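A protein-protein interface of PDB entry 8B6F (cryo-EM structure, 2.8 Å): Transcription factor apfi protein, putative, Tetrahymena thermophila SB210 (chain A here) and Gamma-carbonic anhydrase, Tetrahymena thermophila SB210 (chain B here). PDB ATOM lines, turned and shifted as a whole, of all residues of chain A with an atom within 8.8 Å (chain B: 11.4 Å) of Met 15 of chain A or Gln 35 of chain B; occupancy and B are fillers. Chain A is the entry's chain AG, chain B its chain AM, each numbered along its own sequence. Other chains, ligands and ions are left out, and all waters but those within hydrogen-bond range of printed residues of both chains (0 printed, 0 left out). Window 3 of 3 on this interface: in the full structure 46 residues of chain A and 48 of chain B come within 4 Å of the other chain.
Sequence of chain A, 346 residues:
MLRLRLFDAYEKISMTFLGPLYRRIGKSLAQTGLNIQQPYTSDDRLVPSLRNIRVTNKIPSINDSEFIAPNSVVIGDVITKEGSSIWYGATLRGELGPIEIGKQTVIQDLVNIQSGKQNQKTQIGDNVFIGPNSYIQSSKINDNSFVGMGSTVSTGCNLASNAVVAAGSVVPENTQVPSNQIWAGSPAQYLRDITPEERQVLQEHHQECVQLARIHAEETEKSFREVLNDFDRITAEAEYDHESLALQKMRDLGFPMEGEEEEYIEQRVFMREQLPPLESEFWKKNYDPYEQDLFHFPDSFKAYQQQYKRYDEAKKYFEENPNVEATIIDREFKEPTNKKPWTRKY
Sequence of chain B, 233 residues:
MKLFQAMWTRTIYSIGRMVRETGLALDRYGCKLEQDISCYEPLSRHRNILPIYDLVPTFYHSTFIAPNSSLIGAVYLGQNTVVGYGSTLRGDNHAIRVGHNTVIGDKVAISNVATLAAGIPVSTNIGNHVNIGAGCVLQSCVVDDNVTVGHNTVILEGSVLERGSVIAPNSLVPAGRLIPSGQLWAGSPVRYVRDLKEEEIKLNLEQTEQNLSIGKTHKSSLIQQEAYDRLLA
NH1 of Arg 23 of chain A lies within salt-bridge range of OD1 of Asp 27 of chain B (3.3 Å). NH1 of Arg 23 of chain A sits at hydrogen-bond distance from SG of Cys 31 of chain B (2.7 Å). NE of Arg 23 of chain A lies within salt-bridge range of OE1 of Glu 34 of chain B. The side-chain carboxylate (OD2) of Asp 36 of chain B lies within salt-bridge range of the guanidinium group (NH2) of Arg 23 of chain A (3.2 Å). NH1 of Arg 23 of chain A sits at hydrogen-bond distance from OG of Ser 38 of chain B (3.2 Å).
The backbone carbonyl oxygen of Ser 14 of chain A sits at hydrogen-bond distance from the backbone NH of Gly 19 of chain A (3.2 Å). The backbone carbonyl oxygen of Asp 27 of chain B is in hydrogen-bond range of the side-chain sulfur of Cys 31 of chain B (3.3 Å). The backbone NH (N) of Asp 36 of chain B lies within hydrogen-bond range of the backbone carbonyl oxygen (O) of Cys 31 of chain B (3.0 Å). The side-chain sulfur of Cys 31 of chain B sits at hydrogen-bond distance from the side-chain hydroxyl of Ser 38 of chain B. The side-chain carboxylate (OD1) of Asp 36 of chain B sits at hydrogen-bond distance from the backbone NH (N) of Ser 38 of chain B, 2.6 Å away.
Met 15 of chain A touches Leu 33 of chain B. Met 15 of chain A touches Glu 34 of chain B. Met 15 of chain A touches Gln 35 of chain B (CE to NE2, 3.2 Å). Gly 30 of chain B touches Gly 19 of chain A. Glu 34 of chain B touches Pro 20 of chain A (OE2 to CG, 3.5 Å). Gly 30 of chain B touches Arg 23 of chain A. CD1 of Ile 37 of chain B touches NH1 of Arg 225 of chain A, 3.2 Å away.
Met 15 of chain A touches three residues of chain B. Of chain A, only Met 15 comes within 4 Å of Gln 35 of chain B. No residue of chain B comes within 4 Å of Ser 14 of chain A. Thr 16 of chain A touches none of the printed residues of chain B. No residue of chain B comes within 4 Å of Leu 18 of chain A. Of chain B, only Gly 30 comes within 4 Å of Gly 19 of chain A. Printed residues of chain B within 4 Å of Arg 23 of chain A: Asp 27 (3.3 Å), Gly 30 (3.8 Å), Cys 31 (2.7 Å), Glu 34 (3.3 Å), Asp 36 (3.2 Å) and Ser 38 (3.2 Å). Of the printed residues of chain A, Asp 27 of chain B touches Arg 23. Of the printed residues of chain A, Gly 30 of chain B touches Gly 19 and Arg 23. Phe 17 of chain A touches none of the printed residues of chain B. Tyr 10 of chain A touches none of the printed residues of chain B.
Of the 16 printed residues of chain A, 5 touch a printed residue of chain B. Hydrophobic or aromatic side chains of chain A within 4 Å of the printed part of chain B: Met 15 and Pro 20. Among the printed residues, Asp or Glu carboxylates within 4 Å of a Lys or Arg side-chain nitrogen of the other chain: Arg 23 of chain A with Asp 27 of chain B, Arg 23 of chain A with Glu 34 of chain B and Arg 23 of chain A with Asp 36 of chain B.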
ATOM      1  N   ASP A   8      17.653 -38.470 -31.443  1.00  0.00           N
ATOM      2  CA  ASP A   8      16.597 -37.466 -31.508  1.00  0.00           C
ATOM      3  C   ASP A   8      15.384 -37.885 -30.687  1.00  0.00           C
ATOM      4  O   ASP A   8      14.776 -37.057 -29.999  1.00  0.00           O
ATOM      5  CB  ASP A   8      16.199 -37.214 -32.961  1.00  0.00           C
ATOM      6  CG  ASP A   8      17.257 -36.449 -33.727  1.00  0.00           C
ATOM      7  OD1 ASP A   8      18.305 -37.043 -34.055  1.00  0.00           O
ATOM      8  OD2 ASP A   8      17.043 -35.249 -33.998  1.00  0.00           O
ATOM      9  N   ALA A   9      15.013 -39.164 -30.752  1.00  0.00           N
ATOM     10  CA  ALA A   9      13.883 -39.640 -29.964  1.00  0.00           C
ATOM     11  C   ALA A   9      14.139 -39.464 -28.475  1.00  0.00           C
ATOM     12  O   ALA A   9      13.253 -39.023 -27.733  1.00  0.00           O
ATOM     13  CB  ALA A   9      13.598 -41.106 -30.289  1.00  0.00           C
ATOM     14  N   TYR A  10      15.346 -39.801 -28.015  1.00  0.00           N
ATOM     15  CA  TYR A  10      15.664 -39.633 -26.603  1.00  0.00           C
ATOM     16  C   TYR A  10      15.694 -38.160 -26.214  1.00  0.00           C
ATOM     17  O   TYR A  10      15.242 -37.794 -25.124  1.00  0.00           O
ATOM     18  CB  TYR A  10      17.002 -40.291 -26.271  1.00  0.00           C
ATOM     19  CG  TYR A  10      17.322 -40.248 -24.794  1.00  0.00           C
ATOM     20  CD1 TYR A  10      17.951 -39.144 -24.230  1.00  0.00           C
ATOM     21  CD2 TYR A  10      16.984 -41.306 -23.963  1.00  0.00           C
ATOM     22  CE1 TYR A  10      18.238 -39.098 -22.880  1.00  0.00           C
ATOM     23  CE2 TYR A  10      17.265 -41.271 -22.612  1.00  0.00           C
ATOM     24  CZ  TYR A  10      17.893 -40.165 -22.077  1.00  0.00           C
ATOM     25  OH  TYR A  10      18.177 -40.128 -20.732  1.00  0.00           O
ATOM     26  N   GLU A  11      16.224 -37.300 -27.086  1.00  0.00           N
ATOM     27  CA  GLU A  11      16.231 -35.872 -26.788  1.00  0.00           C
ATOM     28  C   GLU A  11      14.812 -35.357 -26.590  1.00  0.00           C
ATOM     29  O   GLU A  11      14.524 -34.659 -25.612  1.00  0.00           O
ATOM     30  CB  GLU A  11      16.928 -35.105 -27.914  1.00  0.00           C
ATOM     31  CG  GLU A  11      18.439 -35.280 -27.949  1.00  0.00           C
ATOM     32  CD  GLU A  11      19.135 -34.610 -26.779  1.00  0.00           C
ATOM     33  OE1 GLU A  11      18.467 -33.865 -26.034  1.00  0.00           O
ATOM     34  OE2 GLU A  11      20.352 -34.829 -26.606  1.00  0.00           O
ATOM     35  N   LYS A  12      13.911 -35.688 -27.516  1.00  0.00           N
ATOM     36  CA  LYS A  12      12.529 -35.242 -27.382  1.00  0.00           C
ATOM     37  C   LYS A  12      11.886 -35.822 -26.128  1.00  0.00           C
ATOM     38  O   LYS A  12      11.199 -35.111 -25.389  1.00  0.00           O
ATOM     39  CB  LYS A  12      11.730 -35.630 -28.626  1.00  0.00           C
ATOM     40  CG  LYS A  12      12.069 -34.801 -29.857  1.00  0.00           C
ATOM     41  CD  LYS A  12      11.213 -35.200 -31.049  1.00  0.00           C
ATOM     42  CE  LYS A  12      11.440 -34.271 -32.234  1.00  0.00           C
ATOM     43  NZ  LYS A  12      12.864 -34.247 -32.672  1.00  0.00           N
ATOM     44  N   ILE A  13      12.098 -37.116 -25.874  1.00  0.00           N
ATOM     45  CA  ILE A  13      11.484 -37.752 -24.710  1.00  0.00           C
ATOM     46  C   ILE A  13      11.963 -37.086 -23.428  1.00  0.00           C
ATOM     47  O   ILE A  13      11.164 -36.762 -22.540  1.00  0.00           O
ATOM     48  CB  ILE A  13      11.783 -39.263 -24.706  1.00  0.00           C
ATOM     49  CG1 ILE A  13      10.991 -39.961 -25.815  1.00  0.00           C
ATOM     50  CG2 ILE A  13      11.451 -39.884 -23.347  1.00  0.00           C
ATOM     51  CD1 ILE A  13      11.394 -41.406 -26.048  1.00  0.00           C
ATOM     52  N   SER A  14      13.274 -36.876 -23.303  1.00  0.00           N
ATOM     53  CA  SER A  14      13.797 -36.224 -22.108  1.00  0.00           C
ATOM     54  C   SER A  14      13.193 -34.835 -21.946  1.00  0.00           C
ATOM     55  O   SER A  14      12.641 -34.502 -20.891  1.00  0.00           O
ATOM     56  CB  SER A  14      15.323 -36.149 -22.171  1.00  0.00           C
ATOM     57  OG  SER A  14      15.753 -35.320 -23.235  1.00  0.00           O
ATOM     58  N   MET A  15      13.307 -34.002 -22.983  1.00  0.00           N
ATOM     59  CA  MET A  15      12.861 -32.618 -22.874  1.00  0.00           C
ATOM     60  C   MET A  15      11.372 -32.519 -22.562  1.00  0.00           C
ATOM     61  O   MET A  15      10.948 -31.584 -21.874  1.00  0.00           O
ATOM     62  CB  MET A  15      13.174 -31.880 -24.174  1.00  0.00           C
ATOM     63  CG  MET A  15      12.870 -30.391 -24.141  1.00  0.00           C
ATOM     64  SD  MET A  15      13.148 -29.583 -25.731  1.00  0.00           S
ATOM     65  CE  MET A  15      14.874 -29.960 -26.018  1.00  0.00           C
ATOM     66  N   THR A  16      10.565 -33.461 -23.054  1.00  0.00           N
ATOM     67  CA  THR A  16       9.118 -33.358 -22.910  1.00  0.00           C
ATOM     68  C   THR A  16       8.571 -34.102 -21.700  1.00  0.00           C
ATOM     69  O   THR A  16       7.458 -33.796 -21.258  1.00  0.00           O
ATOM     70  CB  THR A  16       8.429 -33.882 -24.179  1.00  0.00           C
ATOM     71  OG1 THR A  16       8.898 -33.151 -25.319  1.00  0.00           O
ATOM     72  CG2 THR A  16       6.911 -33.733 -24.089  1.00  0.00           C
ATOM     73  N   PHE A  17       9.319 -35.053 -21.143  1.00  0.00           N
ATOM     74  CA  PHE A  17       8.832 -35.853 -20.027  1.00  0.00           C
ATOM     75  C   PHE A  17       9.662 -35.669 -18.768  1.00  0.00           C
ATOM     76  O   PHE A  17       9.105 -35.393 -17.701  1.00  0.00           O
ATOM     77  CB  PHE A  17       8.803 -37.339 -20.427  1.00  0.00           C
ATOM     78  CG  PHE A  17       8.204 -38.237 -19.383  1.00  0.00           C
ATOM     79  CD1 PHE A  17       6.830 -38.371 -19.271  1.00  0.00           C
ATOM     80  CD2 PHE A  17       9.015 -38.957 -18.522  1.00  0.00           C
ATOM     81  CE1 PHE A  17       6.276 -39.200 -18.313  1.00  0.00           C
ATOM     82  CE2 PHE A  17       8.469 -39.786 -17.563  1.00  0.00           C
ATOM     83  CZ  PHE A  17       7.098 -39.909 -17.457  1.00  0.00           C
ATOM     84  N   LEU A  18      10.985 -35.816 -18.859  1.00  0.00           N
ATOM     85  CA  LEU A  18      11.804 -35.794 -17.652  1.00  0.00           C
ATOM     86  C   LEU A  18      11.927 -34.384 -17.095  1.00  0.00           C
ATOM     87  O   LEU A  18      11.901 -34.189 -15.874  1.00  0.00           O
ATOM     88  CB  LEU A  18      13.186 -36.378 -17.941  1.00  0.00           C
ATOM     89  CG  LEU A  18      13.207 -37.822 -18.447  1.00  0.00           C
ATOM     90  CD1 LEU A  18      14.629 -38.252 -18.747  1.00  0.00           C
ATOM     91  CD2 LEU A  18      12.561 -38.766 -17.446  1.00  0.00           C
ATOM     92  N   GLY A  19      12.058 -33.390 -17.967  1.00  0.00           N
ATOM     93  CA  GLY A  19      12.161 -32.017 -17.538  1.00  0.00           C
ATOM     94  C   GLY A  19      10.999 -31.615 -16.656  1.00  0.00           C
ATOM     95  O   GLY A  19      11.170 -31.251 -15.490  1.00  0.00           O
ATOM     96  N   PRO A  20       9.783 -31.678 -17.203  1.00  0.00           N
ATOM     97  CA  PRO A  20       8.609 -31.314 -16.393  1.00  0.00           C
ATOM     98  C   PRO A  20       8.468 -32.138 -15.128  1.00  0.00           C
ATOM     99  O   PRO A  20       8.101 -31.595 -14.079  1.00  0.00           O
ATOM    100  CB  PRO A  20       7.438 -31.542 -17.359  1.00  0.00           C
ATOM    101  CG  PRO A  20       8.036 -31.426 -18.715  1.00  0.00           C
ATOM    102  CD  PRO A  20       9.423 -31.972 -18.599  1.00  0.00           C
ATOM    103  N   LEU A  21       8.749 -33.440 -15.194  1.00  0.00           N
ATOM    104  CA  LEU A  21       8.595 -34.288 -14.017  1.00  0.00           C
ATOM    105  C   LEU A  21       9.574 -33.887 -12.920  1.00  0.00           C
ATOM    106  O   LEU A  21       9.188 -33.724 -11.757  1.00  0.00           O
ATOM    107  CB  LEU A  21       8.784 -35.756 -14.402  1.00  0.00           C
ATOM    108  CG  LEU A  21       8.606 -36.777 -13.273  1.00  0.00           C
ATOM    109  CD1 LEU A  21       7.180 -36.760 -12.740  1.00  0.00           C
ATOM    110  CD2 LEU A  21       8.980 -38.166 -13.754  1.00  0.00           C
ATOM    111  N   ARG A  23      11.044 -31.019 -12.602  1.00  0.00           N
ATOM    112  CA  ARG A  23      10.678 -29.684 -12.147  1.00  0.00           C
ATOM    113  C   ARG A  23       9.556 -29.747 -11.118  1.00  0.00           C
ATOM    114  O   ARG A  23       9.631 -29.110 -10.062  1.00  0.00           O
ATOM    115  CB  ARG A  23      10.264 -28.824 -13.341  1.00  0.00           C
ATOM    116  CG  ARG A  23      11.386 -28.560 -14.327  1.00  0.00           C
ATOM    117  CD  ARG A  23      11.843 -27.116 -14.278  1.00  0.00           C
ATOM    118  NE  ARG A  23      10.927 -26.226 -14.977  1.00  0.00           N
ATOM    119  CZ  ARG A  23      10.939 -24.904 -14.873  1.00  0.00           C
ATOM    120  NH1 ARG A  23      11.785 -24.282 -14.069  1.00  0.00           N
ATOM    121  NH2 ARG A  23      10.075 -24.189 -15.587  1.00  0.00           N
ATOM    122  N   ARG A 225      17.878 -11.751 -20.437  1.00  0.00           N
ATOM    123  CA  ARG A 225      18.612 -12.424 -21.502  1.00  0.00           C
ATOM    124  C   ARG A 225      19.932 -11.722 -21.786  1.00  0.00           C
ATOM    125  O   ARG A 225      20.955 -12.376 -22.018  1.00  0.00           O
ATOM    126  CB  ARG A 225      17.752 -12.492 -22.764  1.00  0.00           C
ATOM    127  CG  ARG A 225      16.420 -13.197 -22.555  1.00  0.00           C
ATOM    128  CD  ARG A 225      15.704 -13.431 -23.876  1.00  0.00           C
ATOM    129  NE  ARG A 225      14.388 -14.027 -23.683  1.00  0.00           N
ATOM    130  CZ  ARG A 225      14.168 -15.322 -23.503  1.00  0.00           C
ATOM    131  NH1 ARG A 225      15.161 -16.193 -23.469  1.00  0.00           N
ATOM    132  NH2 ARG A 225      12.920 -15.754 -23.350  1.00  0.00           N
ATOM    133  N   LEU B  26      16.868 -30.436  -7.940  1.00  0.00           N
ATOM    134  CA  LEU B  26      16.064 -31.153  -8.924  1.00  0.00           C
ATOM    135  C   LEU B  26      15.404 -30.191  -9.901  1.00  0.00           C
ATOM    136  O   LEU B  26      15.348 -30.459 -11.105  1.00  0.00           O
ATOM    137  CB  LEU B  26      15.007 -32.008  -8.222  1.00  0.00           C
ATOM    138  CG  LEU B  26      15.290 -33.508  -8.118  1.00  0.00           C
ATOM    139  CD1 LEU B  26      14.229 -34.185  -7.270  1.00  0.00           C
ATOM    140  CD2 LEU B  26      15.353 -34.152  -9.493  1.00  0.00           C
ATOM    141  N   ASP B  27      14.903 -29.060  -9.402  1.00  0.00           N
ATOM    142  CA  ASP B  27      14.298 -28.074 -10.289  1.00  0.00           C
ATOM    143  C   ASP B  27      15.320 -27.533 -11.280  1.00  0.00           C
ATOM    144  O   ASP B  27      15.016 -27.369 -12.467  1.00  0.00           O
ATOM    145  CB  ASP B  27      13.684 -26.941  -9.468  1.00  0.00           C
ATOM    146  CG  ASP B  27      12.775 -26.053 -10.291  1.00  0.00           C
ATOM    147  OD1 ASP B  27      13.152 -25.695 -11.425  1.00  0.00           O
ATOM    148  OD2 ASP B  27      11.675 -25.719  -9.809  1.00  0.00           O
ATOM    149  N   ARG B  28      16.535 -27.240 -10.813  1.00  0.00           N
ATOM    150  CA  ARG B  28      17.574 -26.761 -11.717  1.00  0.00           C
ATOM    151  C   ARG B  28      17.917 -27.810 -12.765  1.00  0.00           C
ATOM    152  O   ARG B  28      18.088 -27.487 -13.945  1.00  0.00           O
ATOM    153  CB  ARG B  28      18.824 -26.367 -10.934  1.00  0.00           C
ATOM    154  CG  ARG B  28      18.775 -24.963 -10.364  1.00  0.00           C
ATOM    155  CD  ARG B  28      20.173 -24.374 -10.261  1.00  0.00           C
ATOM    156  NE  ARG B  28      20.138 -22.956  -9.927  1.00  0.00           N
ATOM    157  CZ  ARG B  28      21.179 -22.140 -10.022  1.00  0.00           C
ATOM    158  NH1 ARG B  28      22.359 -22.569 -10.440  1.00  0.00           N
ATOM    159  NH2 ARG B  28      21.030 -20.860  -9.695  1.00  0.00           N
ATOM    160  N   TYR B  29      18.023 -29.074 -12.355  1.00  0.00           N
ATOM    161  CA  TYR B  29      18.330 -30.135 -13.307  1.00  0.00           C
ATOM    162  C   TYR B  29      17.210 -30.291 -14.326  1.00  0.00           C
ATOM    163  O   TYR B  29      17.466 -30.522 -15.513  1.00  0.00           O
ATOM    164  CB  TYR B  29      18.577 -31.449 -12.569  1.00  0.00           C
ATOM    165  CG  TYR B  29      18.969 -32.586 -13.483  1.00  0.00           C
ATOM    166  CD1 TYR B  29      20.216 -32.613 -14.091  1.00  0.00           C
ATOM    167  CD2 TYR B  29      18.096 -33.636 -13.727  1.00  0.00           C
ATOM    168  CE1 TYR B  29      20.581 -33.649 -14.923  1.00  0.00           C
ATOM    169  CE2 TYR B  29      18.451 -34.677 -14.558  1.00  0.00           C
ATOM    170  CZ  TYR B  29      19.696 -34.678 -15.152  1.00  0.00           C
ATOM    171  OH  TYR B  29      20.053 -35.717 -15.980  1.00  0.00           O
ATOM    172  N   GLY B  30      15.960 -30.166 -13.881  1.00  0.00           N
ATOM    173  CA  GLY B  30      14.846 -30.208 -14.812  1.00  0.00           C
ATOM    174  C   GLY B  30      14.889 -29.068 -15.811  1.00  0.00           C
ATOM    175  O   GLY B  30      14.610 -29.258 -16.997  1.00  0.00           O
ATOM    176  N   CYS B  31      15.242 -27.868 -15.346  1.00  0.00           N
ATOM    177  CA  CYS B  31      15.414 -26.742 -16.259  1.00  0.00           C
ATOM    178  C   CYS B  31      16.503 -27.031 -17.283  1.00  0.00           C
ATOM    179  O   CYS B  31      16.338 -26.743 -18.473  1.00  0.00           O
ATOM    180  CB  CYS B  31      15.749 -25.475 -15.473  1.00  0.00           C
ATOM    181  SG  CYS B  31      14.388 -24.819 -14.490  1.00  0.00           S
ATOM    182  N   LYS B  32      17.624 -27.601 -16.840  1.00  0.00           N
ATOM    183  CA  LYS B  32      18.705 -27.931 -17.763  1.00  0.00           C
ATOM    184  C   LYS B  32      18.235 -28.923 -18.817  1.00  0.00           C
ATOM    185  O   LYS B  32      18.599 -28.812 -19.993  1.00  0.00           O
ATOM    186  CB  LYS B  32      19.902 -28.489 -16.994  1.00  0.00           C
ATOM    187  CG  LYS B  32      20.556 -27.484 -16.061  1.00  0.00           C
ATOM    188  CD  LYS B  32      21.578 -28.152 -15.153  1.00  0.00           C
ATOM    189  CE  LYS B  32      22.088 -27.187 -14.093  1.00  0.00           C
ATOM    190  NZ  LYS B  32      23.003 -27.859 -13.127  1.00  0.00           N
ATOM    191  N   LEU B  33      17.421 -29.900 -18.417  1.00  0.00           N
ATOM    192  CA  LEU B  33      16.953 -30.909 -19.360  1.00  0.00           C
ATOM    193  C   LEU B  33      15.903 -30.332 -20.300  1.00  0.00           C
ATOM    194  O   LEU B  33      15.773 -30.792 -21.439  1.00  0.00           O
ATOM    195  CB  LEU B  33      16.379 -32.107 -18.602  1.00  0.00           C
ATOM    196  CG  LEU B  33      17.353 -33.111 -17.979  1.00  0.00           C
ATOM    197  CD1 LEU B  33      16.583 -34.276 -17.387  1.00  0.00           C
ATOM    198  CD2 LEU B  33      18.377 -33.623 -18.980  1.00  0.00           C
ATOM    199  N   GLU B  34      15.153 -29.336 -19.841  1.00  0.00           N
ATOM    200  CA  GLU B  34      14.046 -28.752 -20.588  1.00  0.00           C
ATOM    201  C   GLU B  34      14.470 -27.555 -21.428  1.00  0.00           C
ATOM    202  O   GLU B  34      13.622 -26.955 -22.098  1.00  0.00           O
ATOM    203  CB  GLU B  34      12.947 -28.318 -19.614  1.00  0.00           C
ATOM    204  CG  GLU B  34      11.534 -28.544 -20.100  1.00  0.00           C
ATOM    205  CD  GLU B  34      10.508 -28.094 -19.082  1.00  0.00           C
ATOM    206  OE1 GLU B  34      10.918 -27.612 -18.006  1.00  0.00           O
ATOM    207  OE2 GLU B  34       9.296 -28.216 -19.354  1.00  0.00           O
ATOM    208  N   GLN B  35      15.753 -27.194 -21.411  1.00  0.00           N
ATOM    209  CA  GLN B  35      16.252 -26.004 -22.103  1.00  0.00           C
ATOM    210  C   GLN B  35      15.523 -24.747 -21.629  1.00  0.00           C
ATOM    211  O   GLN B  35      15.110 -23.905 -22.429  1.00  0.00           O
ATOM    212  CB  GLN B  35      16.141 -26.171 -23.620  1.00  0.00           C
ATOM    213  CG  GLN B  35      16.851 -27.416 -24.127  1.00  0.00           C
ATOM    214  CD  GLN B  35      16.935 -27.476 -25.637  1.00  0.00           C
ATOM    215  OE1 GLN B  35      16.308 -26.687 -26.341  1.00  0.00           O
ATOM    216  NE2 GLN B  35      17.709 -28.430 -26.146  1.00  0.00           N
ATOM    217  N   ASP B  36      15.346 -24.640 -20.316  1.00  0.00           N
ATOM    218  CA  ASP B  36      14.669 -23.521 -19.672  1.00  0.00           C
ATOM    219  C   ASP B  36      15.697 -22.701 -18.897  1.00  0.00           C
ATOM    220  O   ASP B  36      16.507 -23.266 -18.158  1.00  0.00           O
ATOM    221  CB  ASP B  36      13.566 -24.047 -18.753  1.00  0.00           C
ATOM    222  CG  ASP B  36      12.733 -22.946 -18.146  1.00  0.00           C
ATOM    223  OD1 ASP B  36      13.306 -21.980 -17.604  1.00  0.00           O
ATOM    224  OD2 ASP B  36      11.493 -23.054 -18.212  1.00  0.00           O
ATOM    225  N   ILE B  37      15.670 -21.377 -19.067  1.00  0.00           N
ATOM    226  CA  ILE B  37      16.666 -20.488 -18.463  1.00  0.00           C
ATOM    227  C   ILE B  37      16.149 -19.804 -17.193  1.00  0.00           C
ATOM    228  O   ILE B  37      16.809 -18.903 -16.671  1.00  0.00           O
ATOM    229  CB  ILE B  37      17.201 -19.461 -19.473  1.00  0.00           C
ATOM    230  CG1 ILE B  37      16.067 -18.717 -20.168  1.00  0.00           C
ATOM    231  CG2 ILE B  37      18.103 -20.147 -20.493  1.00  0.00           C
ATOM    232  CD1 ILE B  37      16.545 -17.508 -20.938  1.00  0.00           C
ATOM    233  N   SER B  38      14.981 -20.207 -16.690  1.00  0.00           N
ATOM    234  CA  SER B  38      14.333 -19.506 -15.581  1.00  0.00           C
ATOM    235  C   SER B  38      15.199 -19.521 -14.322  1.00  0.00           C
ATOM    236  O   SER B  38      15.291 -18.515 -13.609  1.00  0.00           O
ATOM    237  CB  SER B  38      12.962 -20.118 -15.303  1.00  0.00           C
ATOM    238  OG  SER B  38      13.078 -21.464 -14.883  1.00  0.00           O
ATOM    239  N   CYS B  39      15.841 -20.654 -14.038  1.00  0.00           N
ATOM    240  CA  CYS B  39      16.656 -20.810 -12.833  1.00  0.00           C
ATOM    241  C   CYS B  39      17.836 -19.845 -12.838  1.00  0.00           C
ATOM    242  O   CYS B  39      18.208 -19.300 -11.792  1.00  0.00           O
ATOM    243  CB  CYS B  39      17.145 -22.254 -12.713  1.00  0.00           C
ATOM    244  SG  CYS B  39      17.816 -22.949 -14.239  1.00  0.00           S
ATOM    245  N   TYR B  40      18.433 -19.623 -14.005  1.00  0.00           N
ATOM    246  CA  TYR B  40      19.647 -18.826 -14.144  1.00  0.00           C
ATOM    247  C   TYR B  40      19.448 -17.363 -13.762  1.00  0.00           C
ATOM    248  O   TYR B  40      20.430 -16.691 -13.435  1.00  0.00           O
ATOM    249  CB  TYR B  40      20.159 -18.907 -15.581  1.00  0.00           C
ATOM    250  CG  TYR B  40      20.371 -20.317 -16.074  1.00  0.00           C
ATOM    251  CD1 TYR B  40      20.822 -21.314 -15.219  1.00  0.00           C
ATOM    252  CD2 TYR B  40      20.114 -20.652 -17.395  1.00  0.00           C
ATOM    253  CE1 TYR B  40      21.013 -22.605 -15.668  1.00  0.00           C
ATOM    254  CE2 TYR B  40      20.304 -21.939 -17.854  1.00  0.00           C
ATOM    255  CZ  TYR B  40      20.752 -22.911 -16.986  1.00  0.00           C
ATOM    256  OH  TYR B  40      20.941 -24.195 -17.445  1.00  0.00           O
